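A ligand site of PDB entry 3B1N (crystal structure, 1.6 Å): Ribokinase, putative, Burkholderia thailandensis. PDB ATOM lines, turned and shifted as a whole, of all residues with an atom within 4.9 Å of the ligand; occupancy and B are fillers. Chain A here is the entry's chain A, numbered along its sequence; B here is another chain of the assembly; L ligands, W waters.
The side-chain amide nitrogen (ND2) of Asn 111 is in hydrogen-bond range of the backbone carbonyl oxygen (O) of Pro 248 (3.3 Å). The side-chain amide oxygen of Asn 111 sits at hydrogen-bond distance from the side-chain amide nitrogen of Gln 113 (2.8 Å). O of Gly 252 sits at hydrogen-bond distance from NH1 of Arg 256, 2.9 Å away. The side-chain sulfur of Cys 251 lies within hydrogen-bond range of the backbone carbonyl oxygen of Gly 280, at 3.5 Å. SG of Cys 251 is in hydrogen-bond range of O of Pro 248, 3.3 Å away.
The backbone carbonyl oxygen (O) of Gly 225 sits at hydrogen-bond distance from an oxygen (O9) of the ligand (2.8 Å). An oxygen (O4) of the ligand sits at hydrogen-bond distance from the side-chain hydroxyl (OG1) of Thr 220, 2.8 Å away. A ring nitrogen (NE2) of His 31 of chain B sits at hydrogen-bond distance from an oxygen (O5) of the ligand, at 2.8 Å. An oxygen (O1) of the ligand sits at hydrogen-bond distance from the side-chain amide nitrogen (ND2) of Asn 111, 2.8 Å away. The backbone NH (N) of Gly 252 sits at hydrogen-bond distance from an oxygen (O1) of the ligand (2.9 Å). ND2 of Asn 192 lies within hydrogen-bond range of O2 of the ligand, 2.9 Å away. An oxygen (O4) of the ligand lies within hydrogen-bond range of the backbone NH of Gly 222 (3.0 Å). An oxygen (O10) of the ligand lies within hydrogen-bond range of the side-chain hydroxyl (OG) of Ser 277, 3.2 Å away.
N of Arg 221 touches O4 of the ligand (3.6 Å). CB of Glu 223 touches N3 of the ligand, at 3.5 Å. O of Val 240 touches C9 of the ligand, 3.1 Å away. CG2 of Val 245 touches N3 of the ligand, at 3.97 Å. Cys 251 touches the ligand. Phe 255 touches the ligand. Gly 280 touches the ligand. CA of Ala 281 touches N5 of the ligand, at 3.9 Å. Ile 284 touches the ligand (CD1 to N3, 3.5 Å). Hydrophobic or aromatic side chains that line the ligand: Val 245, Phe 255, Ala 281, Ile 284 and His 31 of chain B.
Water W10 lies within hydrogen-bond range of an oxygen (O2) of the ligand (2.7 Å), the backbone carbonyl oxygen (O) of Asn 111 (2.8 Å) and the side-chain amide nitrogen (ND2) of Asn 192 (3.5 Å). Water W3 lies within hydrogen-bond range of OG1 of Thr 220 (2.7 Å), O3 of the ligand (2.7 Å) and NH1 of Arg 256 (2.7 Å). Water W11 lies within hydrogen-bond range of N4 of the ligand (2.8 Å) and N of Ala 242 (2.9 Å). Water W1 lies within hydrogen-bond range of the side-chain amide nitrogen (NE2) of Gln 113, an oxygen (O1) of the ligand and the backbone NH (N) of Gly 250. Water W9 lies within hydrogen-bond range of the side-chain carboxylate (OE1) of Glu 223 and a nitrogen (N3) of the ligand. Water W6 bridges an oxygen (O3) of the ligand (3.2 Å) and the guanidinium group of Arg 256 (3.3 Å).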
ATOM      1  N   ASN A 111      -5.918 -14.293  10.241  1.00  0.00           N
ATOM      2  CA  ASN A 111      -6.391 -14.605   8.869  1.00  0.00           C
ATOM      3  C   ASN A 111      -6.734 -16.074   8.686  1.00  0.00           C
ATOM      4  O   ASN A 111      -6.600 -16.623   7.596  1.00  0.00           O
ATOM      5  CB  ASN A 111      -5.374 -14.166   7.789  1.00  0.00           C
ATOM      6  CG  ASN A 111      -6.027 -13.697   6.507  1.00  0.00           C
ATOM      7  OD1 ASN A 111      -7.261 -13.666   6.379  1.00  0.00           O
ATOM      8  ND2 ASN A 111      -5.182 -13.317   5.531  1.00  0.00           N
ATOM      9  N   GLN A 113      -9.389 -17.821   7.849  1.00  0.00           N
ATOM     10  CA  GLN A 113     -10.667 -17.642   7.215  1.00  0.00           C
ATOM     11  C   GLN A 113     -11.378 -18.956   7.077  1.00  0.00           C
ATOM     12  O   GLN A 113     -10.881 -19.861   6.379  1.00  0.00           O
ATOM     13  CB  GLN A 113     -10.616 -16.998   5.791  1.00  0.00           C
ATOM     14  CG  GLN A 113     -10.112 -15.570   5.826  1.00  0.00           C
ATOM     15  CD  GLN A 113     -10.040 -14.950   4.459  1.00  0.00           C
ATOM     16  OE1 GLN A 113     -10.901 -15.174   3.613  1.00  0.00           O
ATOM     17  NE2 GLN A 113      -9.005 -14.157   4.229  1.00  0.00           N
ATOM     18  N   ASN A 192      -0.744 -18.921   0.191  1.00  0.00           N
ATOM     19  CA  ASN A 192      -0.279 -18.719   1.578  1.00  0.00           C
ATOM     20  C   ASN A 192       0.340 -20.012   2.114  1.00  0.00           C
ATOM     21  O   ASN A 192       0.313 -21.036   1.444  1.00  0.00           O
ATOM     22  CB  ASN A 192      -1.361 -18.098   2.499  1.00  0.00           C
ATOM     23  CG  ASN A 192      -2.454 -19.073   2.915  1.00  0.00           C
ATOM     24  OD1 ASN A 192      -2.315 -20.299   2.857  1.00  0.00           O
ATOM     25  ND2 ASN A 192      -3.569 -18.508   3.366  1.00  0.00           N
ATOM     26  N   THR A 220       3.048 -16.752   0.954  1.00  0.00           N
ATOM     27  CA  THR A 220       2.880 -15.675   1.969  1.00  0.00           C
ATOM     28  C   THR A 220       2.646 -16.268   3.360  1.00  0.00           C
ATOM     29  O   THR A 220       2.007 -17.319   3.541  1.00  0.00           O
ATOM     30  CB  THR A 220       1.740 -14.733   1.615  1.00  0.00           C
ATOM     31  OG1 THR A 220       0.492 -15.420   1.658  1.00  0.00           O
ATOM     32  CG2 THR A 220       1.901 -14.110   0.225  1.00  0.00           C
ATOM     33  N   ARG A 221       3.103 -15.506   4.348  1.00  0.00           N
ATOM     34  CA  ARG A 221       3.217 -16.020   5.699  1.00  0.00           C
ATOM     35  C   ARG A 221       2.709 -15.031   6.727  1.00  0.00           C
ATOM     36  O   ARG A 221       3.255 -14.881   7.809  1.00  0.00           O
ATOM     37  CB  ARG A 221       4.706 -16.340   5.951  1.00  0.00           C
ATOM     38  CG  ARG A 221       5.229 -17.419   4.985  1.00  0.00           C
ATOM     39  CD  ARG A 221       6.718 -17.722   5.286  1.00  0.00           C
ATOM     40  NE  ARG A 221       7.311 -18.488   4.199  1.00  0.00           N
ATOM     41  CZ  ARG A 221       7.205 -19.823   4.041  1.00  0.00           C
ATOM     42  NH1 ARG A 221       6.504 -20.575   4.898  1.00  0.00           N
ATOM     43  NH2 ARG A 221       7.849 -20.406   3.007  1.00  0.00           N
ATOM     44  N   GLY A 222       1.640 -14.335   6.356  1.00  0.00           N
ATOM     45  CA  GLY A 222       0.980 -13.430   7.302  1.00  0.00           C
ATOM     46  C   GLY A 222       1.941 -12.400   7.856  1.00  0.00           C
ATOM     47  O   GLY A 222       2.652 -11.756   7.097  1.00  0.00           O
ATOM     48  N   GLU A 223       1.928 -12.239   9.175  1.00  0.00           N
ATOM     49  CA  GLU A 223       2.790 -11.223   9.830  1.00  0.00           C
ATOM     50  C   GLU A 223       4.292 -11.481   9.633  1.00  0.00           C
ATOM     51  O   GLU A 223       5.101 -10.596   9.886  1.00  0.00           O
ATOM     52  CB  GLU A 223       2.427 -11.057  11.321  1.00  0.00           C
ATOM     53  CG  GLU A 223       2.894 -12.206  12.165  1.00  0.00           C
ATOM     54  CD  GLU A 223       2.563 -11.998  13.659  1.00  0.00           C
ATOM     55  OE1 GLU A 223       2.462 -10.820  14.083  1.00  0.00           O
ATOM     56  OE2 GLU A 223       2.365 -12.992  14.371  1.00  0.00           O
ATOM     57  N   GLY A 225       5.690 -12.081   6.739  1.00  0.00           N
ATOM     58  CA  GLY A 225       6.179 -11.668   5.415  1.00  0.00           C
ATOM     59  C   GLY A 225       5.848 -12.735   4.358  1.00  0.00           C
ATOM     60  O   GLY A 225       4.712 -13.252   4.331  1.00  0.00           O
ATOM     61  N   ALA A 226       6.841 -13.012   3.522  1.00  0.00           N
ATOM     62  CA  ALA A 226       6.623 -13.960   2.401  1.00  0.00           C
ATOM     63  C   ALA A 226       7.955 -14.483   1.956  1.00  0.00           C
ATOM     64  O   ALA A 226       8.987 -13.902   2.259  1.00  0.00           O
ATOM     65  CB  ALA A 226       5.891 -13.283   1.222  1.00  0.00           C
ATOM     66  N   ALA A 239       7.725  -8.527   6.334  1.00  0.00           N
ATOM     67  CA  ALA A 239       6.451  -7.805   6.490  1.00  0.00           C
ATOM     68  C   ALA A 239       6.719  -6.342   6.789  1.00  0.00           C
ATOM     69  O   ALA A 239       7.769  -5.985   7.372  1.00  0.00           O
ATOM     70  CB  ALA A 239       5.583  -8.432   7.650  1.00  0.00           C
ATOM     71  N   VAL A 240       5.785  -5.488   6.414  1.00  0.00           N
ATOM     72  CA  VAL A 240       5.759  -4.119   6.907  1.00  0.00           C
ATOM     73  C   VAL A 240       4.929  -4.092   8.157  1.00  0.00           C
ATOM     74  O   VAL A 240       3.866  -4.698   8.218  1.00  0.00           O
ATOM     75  CB  VAL A 240       5.168  -3.240   5.807  1.00  0.00           C
ATOM     76  CG1 VAL A 240       4.973  -1.758   6.289  1.00  0.00           C
ATOM     77  CG2 VAL A 240       6.028  -3.291   4.542  1.00  0.00           C
ATOM     78  N   ALA A 242       2.187  -3.142  10.449  1.00  0.00           N
ATOM     79  CA  ALA A 242       0.878  -2.523  10.217  1.00  0.00           C
ATOM     80  C   ALA A 242       0.661  -1.369  11.211  1.00  0.00           C
ATOM     81  O   ALA A 242       1.020  -1.452  12.377  1.00  0.00           O
ATOM     82  CB  ALA A 242      -0.228  -3.578  10.410  1.00  0.00           C
ATOM     83  N   VAL A 245      -3.781  -3.701  13.327  1.00  0.00           N
ATOM     84  CA  VAL A 245      -4.241  -4.990  12.792  1.00  0.00           C
ATOM     85  C   VAL A 245      -5.738  -5.099  13.082  1.00  0.00           C
ATOM     86  O   VAL A 245      -6.147  -5.425  14.218  1.00  0.00           O
ATOM     87  CB  VAL A 245      -3.394  -6.167  13.413  1.00  0.00           C
ATOM     88  CG1 VAL A 245      -3.965  -7.547  13.000  1.00  0.00           C
ATOM     89  CG2 VAL A 245      -1.943  -6.050  12.906  1.00  0.00           C
ATOM     90  N   PRO A 248      -7.552  -9.022   8.486  1.00  0.00           N
ATOM     91  CA  PRO A 248      -6.643  -9.481   7.419  1.00  0.00           C
ATOM     92  C   PRO A 248      -7.333  -9.995   6.163  1.00  0.00           C
ATOM     93  O   PRO A 248      -6.637 -10.398   5.220  1.00  0.00           O
ATOM     94  CB  PRO A 248      -5.887 -10.646   8.060  1.00  0.00           C
ATOM     95  CG  PRO A 248      -6.493 -10.935   9.326  1.00  0.00           C
ATOM     96  CD  PRO A 248      -7.582  -9.915   9.667  1.00  0.00           C
ATOM     97  N   GLY A 250      -8.469 -10.366   2.739  1.00  0.00           N
ATOM     98  CA  GLY A 250      -8.064  -9.649   1.516  1.00  0.00           C
ATOM     99  C   GLY A 250      -6.610  -9.309   1.511  1.00  0.00           C
ATOM    100  O   GLY A 250      -6.176  -8.737   0.510  1.00  0.00           O
ATOM    101  N   CYS A 251      -5.857  -9.636   2.586  1.00  0.00           N
ATOM    102  CA  CYS A 251      -4.401  -9.283   2.553  1.00  0.00           C
ATOM    103  C   CYS A 251      -3.659  -9.920   1.399  1.00  0.00           C
ATOM    104  O   CYS A 251      -2.867  -9.244   0.746  1.00  0.00           O
ATOM    105  CB  CYS A 251      -3.699  -9.698   3.865  1.00  0.00           C
ATOM    106  SG  CYS A 251      -3.998  -8.486   5.180  1.00  0.00           S
ATOM    107  N   GLY A 252      -3.908 -11.206   1.148  1.00  0.00           N
ATOM    108  CA  GLY A 252      -3.221 -11.861   0.048  1.00  0.00           C
ATOM    109  C   GLY A 252      -3.576 -11.236  -1.296  1.00  0.00           C
ATOM    110  O   GLY A 252      -2.742 -11.229  -2.191  1.00  0.00           O
ATOM    111  N   PHE A 255      -1.687  -8.031  -1.636  1.00  0.00           N
ATOM    112  CA  PHE A 255      -0.318  -8.475  -1.911  1.00  0.00           C
ATOM    113  C   PHE A 255      -0.180  -8.881  -3.388  1.00  0.00           C
ATOM    114  O   PHE A 255       0.750  -8.422  -4.060  1.00  0.00           O
ATOM    115  CB  PHE A 255       0.007  -9.665  -0.964  1.00  0.00           C
ATOM    116  CG  PHE A 255       1.377 -10.256  -1.145  1.00  0.00           C
ATOM    117  CD1 PHE A 255       2.400  -9.956  -0.242  1.00  0.00           C
ATOM    118  CD2 PHE A 255       1.617 -11.136  -2.203  1.00  0.00           C
ATOM    119  CE1 PHE A 255       3.677 -10.566  -0.424  1.00  0.00           C
ATOM    120  CE2 PHE A 255       2.900 -11.723  -2.406  1.00  0.00           C
ATOM    121  CZ  PHE A 255       3.910 -11.423  -1.522  1.00  0.00           C
ATOM    122  N   ARG A 256      -1.149  -9.640  -3.921  1.00  0.00           N
ATOM    123  CA  ARG A 256      -1.040 -10.055  -5.328  1.00  0.00           C
ATOM    124  C   ARG A 256      -1.132  -8.860  -6.274  1.00  0.00           C
ATOM    125  O   ARG A 256      -0.468  -8.828  -7.302  1.00  0.00           O
ATOM    126  CB  ARG A 256      -2.134 -11.063  -5.671  1.00  0.00           C
ATOM    127  CG  ARG A 256      -1.771 -12.415  -5.131  1.00  0.00           C
ATOM    128  CD  ARG A 256      -3.008 -13.271  -4.863  1.00  0.00           C
ATOM    129  NE  ARG A 256      -2.708 -14.583  -4.362  1.00  0.00           N
ATOM    130  CZ  ARG A 256      -2.168 -14.853  -3.164  1.00  0.00           C
ATOM    131  NH1 ARG A 256      -1.719 -13.899  -2.359  1.00  0.00           N
ATOM    132  NH2 ARG A 256      -2.030 -16.131  -2.813  1.00  0.00           N
ATOM    133  N   ALA A 276       4.362  -5.728  -2.713  1.00  0.00           N
ATOM    134  CA  ALA A 276       3.258  -6.653  -2.345  1.00  0.00           C
ATOM    135  C   ALA A 276       3.068  -6.677  -0.829  1.00  0.00           C
ATOM    136  O   ALA A 276       1.943  -6.572  -0.290  1.00  0.00           O
ATOM    137  CB  ALA A 276       3.588  -8.032  -2.879  1.00  0.00           C
ATOM    138  N   SER A 277       4.182  -6.801  -0.089  1.00  0.00           N
ATOM    139  CA  SER A 277       4.125  -6.813   1.352  1.00  0.00           C
ATOM    140  C   SER A 277       3.533  -5.554   1.911  1.00  0.00           C
ATOM    141  O   SER A 277       2.724  -5.560   2.843  1.00  0.00           O
ATOM    142  CB  SER A 277       5.550  -7.023   1.852  1.00  0.00           C
ATOM    143  OG  SER A 277       5.562  -7.186   3.249  1.00  0.00           O
ATOM    144  N   GLY A 280      -0.238  -5.483   1.508  1.00  0.00           N
ATOM    145  CA  GLY A 280      -0.876  -6.284   2.525  1.00  0.00           C
ATOM    146  C   GLY A 280      -1.000  -5.587   3.882  1.00  0.00           C
ATOM    147  O   GLY A 280      -2.014  -5.714   4.583  1.00  0.00           O
ATOM    148  N   ALA A 281       0.070  -4.882   4.270  1.00  0.00           N
ATOM    149  CA  ALA A 281       0.080  -4.142   5.535  1.00  0.00           C
ATOM    150  C   ALA A 281      -0.868  -2.904   5.508  1.00  0.00           C
ATOM    151  O   ALA A 281      -1.446  -2.588   6.508  1.00  0.00           O
ATOM    152  CB  ALA A 281       1.533  -3.679   5.903  1.00  0.00           C
ATOM    153  N   ILE A 284      -4.497  -4.382   5.992  1.00  0.00           N
ATOM    154  CA  ILE A 284      -4.909  -4.980   7.278  1.00  0.00           C
ATOM    155  C   ILE A 284      -5.366  -3.961   8.309  1.00  0.00           C
ATOM    156  O   ILE A 284      -6.023  -4.330   9.297  1.00  0.00           O
ATOM    157  CB  ILE A 284      -3.770  -5.906   7.871  1.00  0.00           C
ATOM    158  CG1 ILE A 284      -4.343  -6.901   8.853  1.00  0.00           C
ATOM    159  CG2 ILE A 284      -2.616  -5.055   8.454  1.00  0.00           C
ATOM    160  CD1 ILE A 284      -3.315  -8.011   9.240  1.00  0.00           C
ATOM    161  N   HIS B  31      -0.949 -19.575   9.330  1.00  0.00           N
ATOM    162  CA  HIS B  31      -2.407 -19.748   9.252  1.00  0.00           C
ATOM    163  C   HIS B  31      -2.710 -21.130   9.816  1.00  0.00           C
ATOM    164  O   HIS B  31      -2.285 -22.145   9.193  1.00  0.00           O
ATOM    165  CB  HIS B  31      -2.905 -19.610   7.794  1.00  0.00           C
ATOM    166  CG  HIS B  31      -2.499 -18.334   7.128  1.00  0.00           C
ATOM    167  ND1 HIS B  31      -1.253 -18.119   6.559  1.00  0.00           N
ATOM    168  CD2 HIS B  31      -3.194 -17.174   6.968  1.00  0.00           C
ATOM    169  CE1 HIS B  31      -1.192 -16.874   6.093  1.00  0.00           C
ATOM    170  NE2 HIS B  31      -2.356 -16.275   6.354  1.00  0.00           N
HETATM  171  P1  LIG L   1      -3.819 -14.632   2.611  1.00  0.00           P
HETATM  172  O1  LIG L   1      -4.732 -13.402   2.784  1.00  0.00           O
HETATM  173  O2  LIG L   1      -3.990 -15.644   3.691  1.00  0.00           O
HETATM  174  O3  LIG L   1      -3.863 -15.084   1.191  1.00  0.00           O
HETATM  175  P2  LIG L   1      -1.546 -13.625   4.234  1.00  0.00           P
HETATM  176  O4  LIG L   1      -0.326 -14.490   4.140  1.00  0.00           O
HETATM  177  O5  LIG L   1      -2.307 -13.621   5.524  1.00  0.00           O
HETATM  178  O6  LIG L   1      -2.401 -13.923   2.961  1.00  0.00           O
HETATM  179  O7  LIG L   1      -1.144 -12.066   4.031  1.00  0.00           O
HETATM  180  C1  LIG L   1      -0.565 -11.636   2.771  1.00  0.00           C
HETATM  181  C2  LIG L   1       0.533 -10.597   3.072  1.00  0.00           C
HETATM  182  O8  LIG L   1      -0.095  -9.470   3.757  1.00  0.00           O
HETATM  183  C3  LIG L   1       1.638 -11.012   4.037  1.00  0.00           C
HETATM  184  O9  LIG L   1       2.619 -11.768   3.301  1.00  0.00           O
HETATM  185  C4  LIG L   1       2.096  -9.698   4.599  1.00  0.00           C
HETATM  186  O10 LIG L   1       2.960  -9.071   3.653  1.00  0.00           O
HETATM  187  C5  LIG L   1       0.796  -8.862   4.678  1.00  0.00           C
HETATM  188  N1  LIG L   1       0.297  -9.098   6.037  1.00  0.00           N
HETATM  189  C6  LIG L   1      -0.540 -10.095   6.434  1.00  0.00           C
HETATM  190  N2  LIG L   1      -0.792 -10.075   7.775  1.00  0.00           N
HETATM  191  C7  LIG L   1      -0.041  -9.051   8.273  1.00  0.00           C
HETATM  192  C8  LIG L   1       0.217  -8.476   9.587  1.00  0.00           C
HETATM  193  N3  LIG L   1      -0.320  -8.944  10.727  1.00  0.00           N
HETATM  194  N4  LIG L   1       1.092  -7.399   9.640  1.00  0.00           N
HETATM  195  C9  LIG L   1       1.605  -6.867   8.519  1.00  0.00           C
HETATM  196  N5  LIG L   1       1.419  -7.362   7.301  1.00  0.00           N
HETATM  197  C10 LIG L   1       0.615  -8.439   7.139  1.00  0.00           C
HETATM  198  O   HOH W   1      -7.468 -12.988   2.161  1.00  0.00           O
HETATM  199  O   HOH W   2      -5.165 -17.315   0.122  1.00  0.00           O
HETATM  200  O   HOH W   3      -1.496 -15.433  -0.106  1.00  0.00           O
HETATM  201  O   HOH W   4      -2.605 -12.330   8.047  1.00  0.00           O
HETATM  202  O   HOH W   5       3.389  -6.764   5.312  1.00  0.00           O
HETATM  203  O   HOH W   6      -4.979 -14.305  -1.712  1.00  0.00           O
HETATM  204  O   HOH W   7      -1.881 -11.348  11.415  1.00  0.00           O
HETATM  205  O   HOH W   8       5.343 -10.272   2.631  1.00  0.00           O
HETATM  206  O   HOH W   9       0.594  -8.584  13.528  1.00  0.00           O
HETATM  207  O   HOH W  10      -6.135 -16.732   4.839  1.00  0.00           O
HETATM  208  O   HOH W  11       2.279  -5.859  11.591  1.00  0.00           O
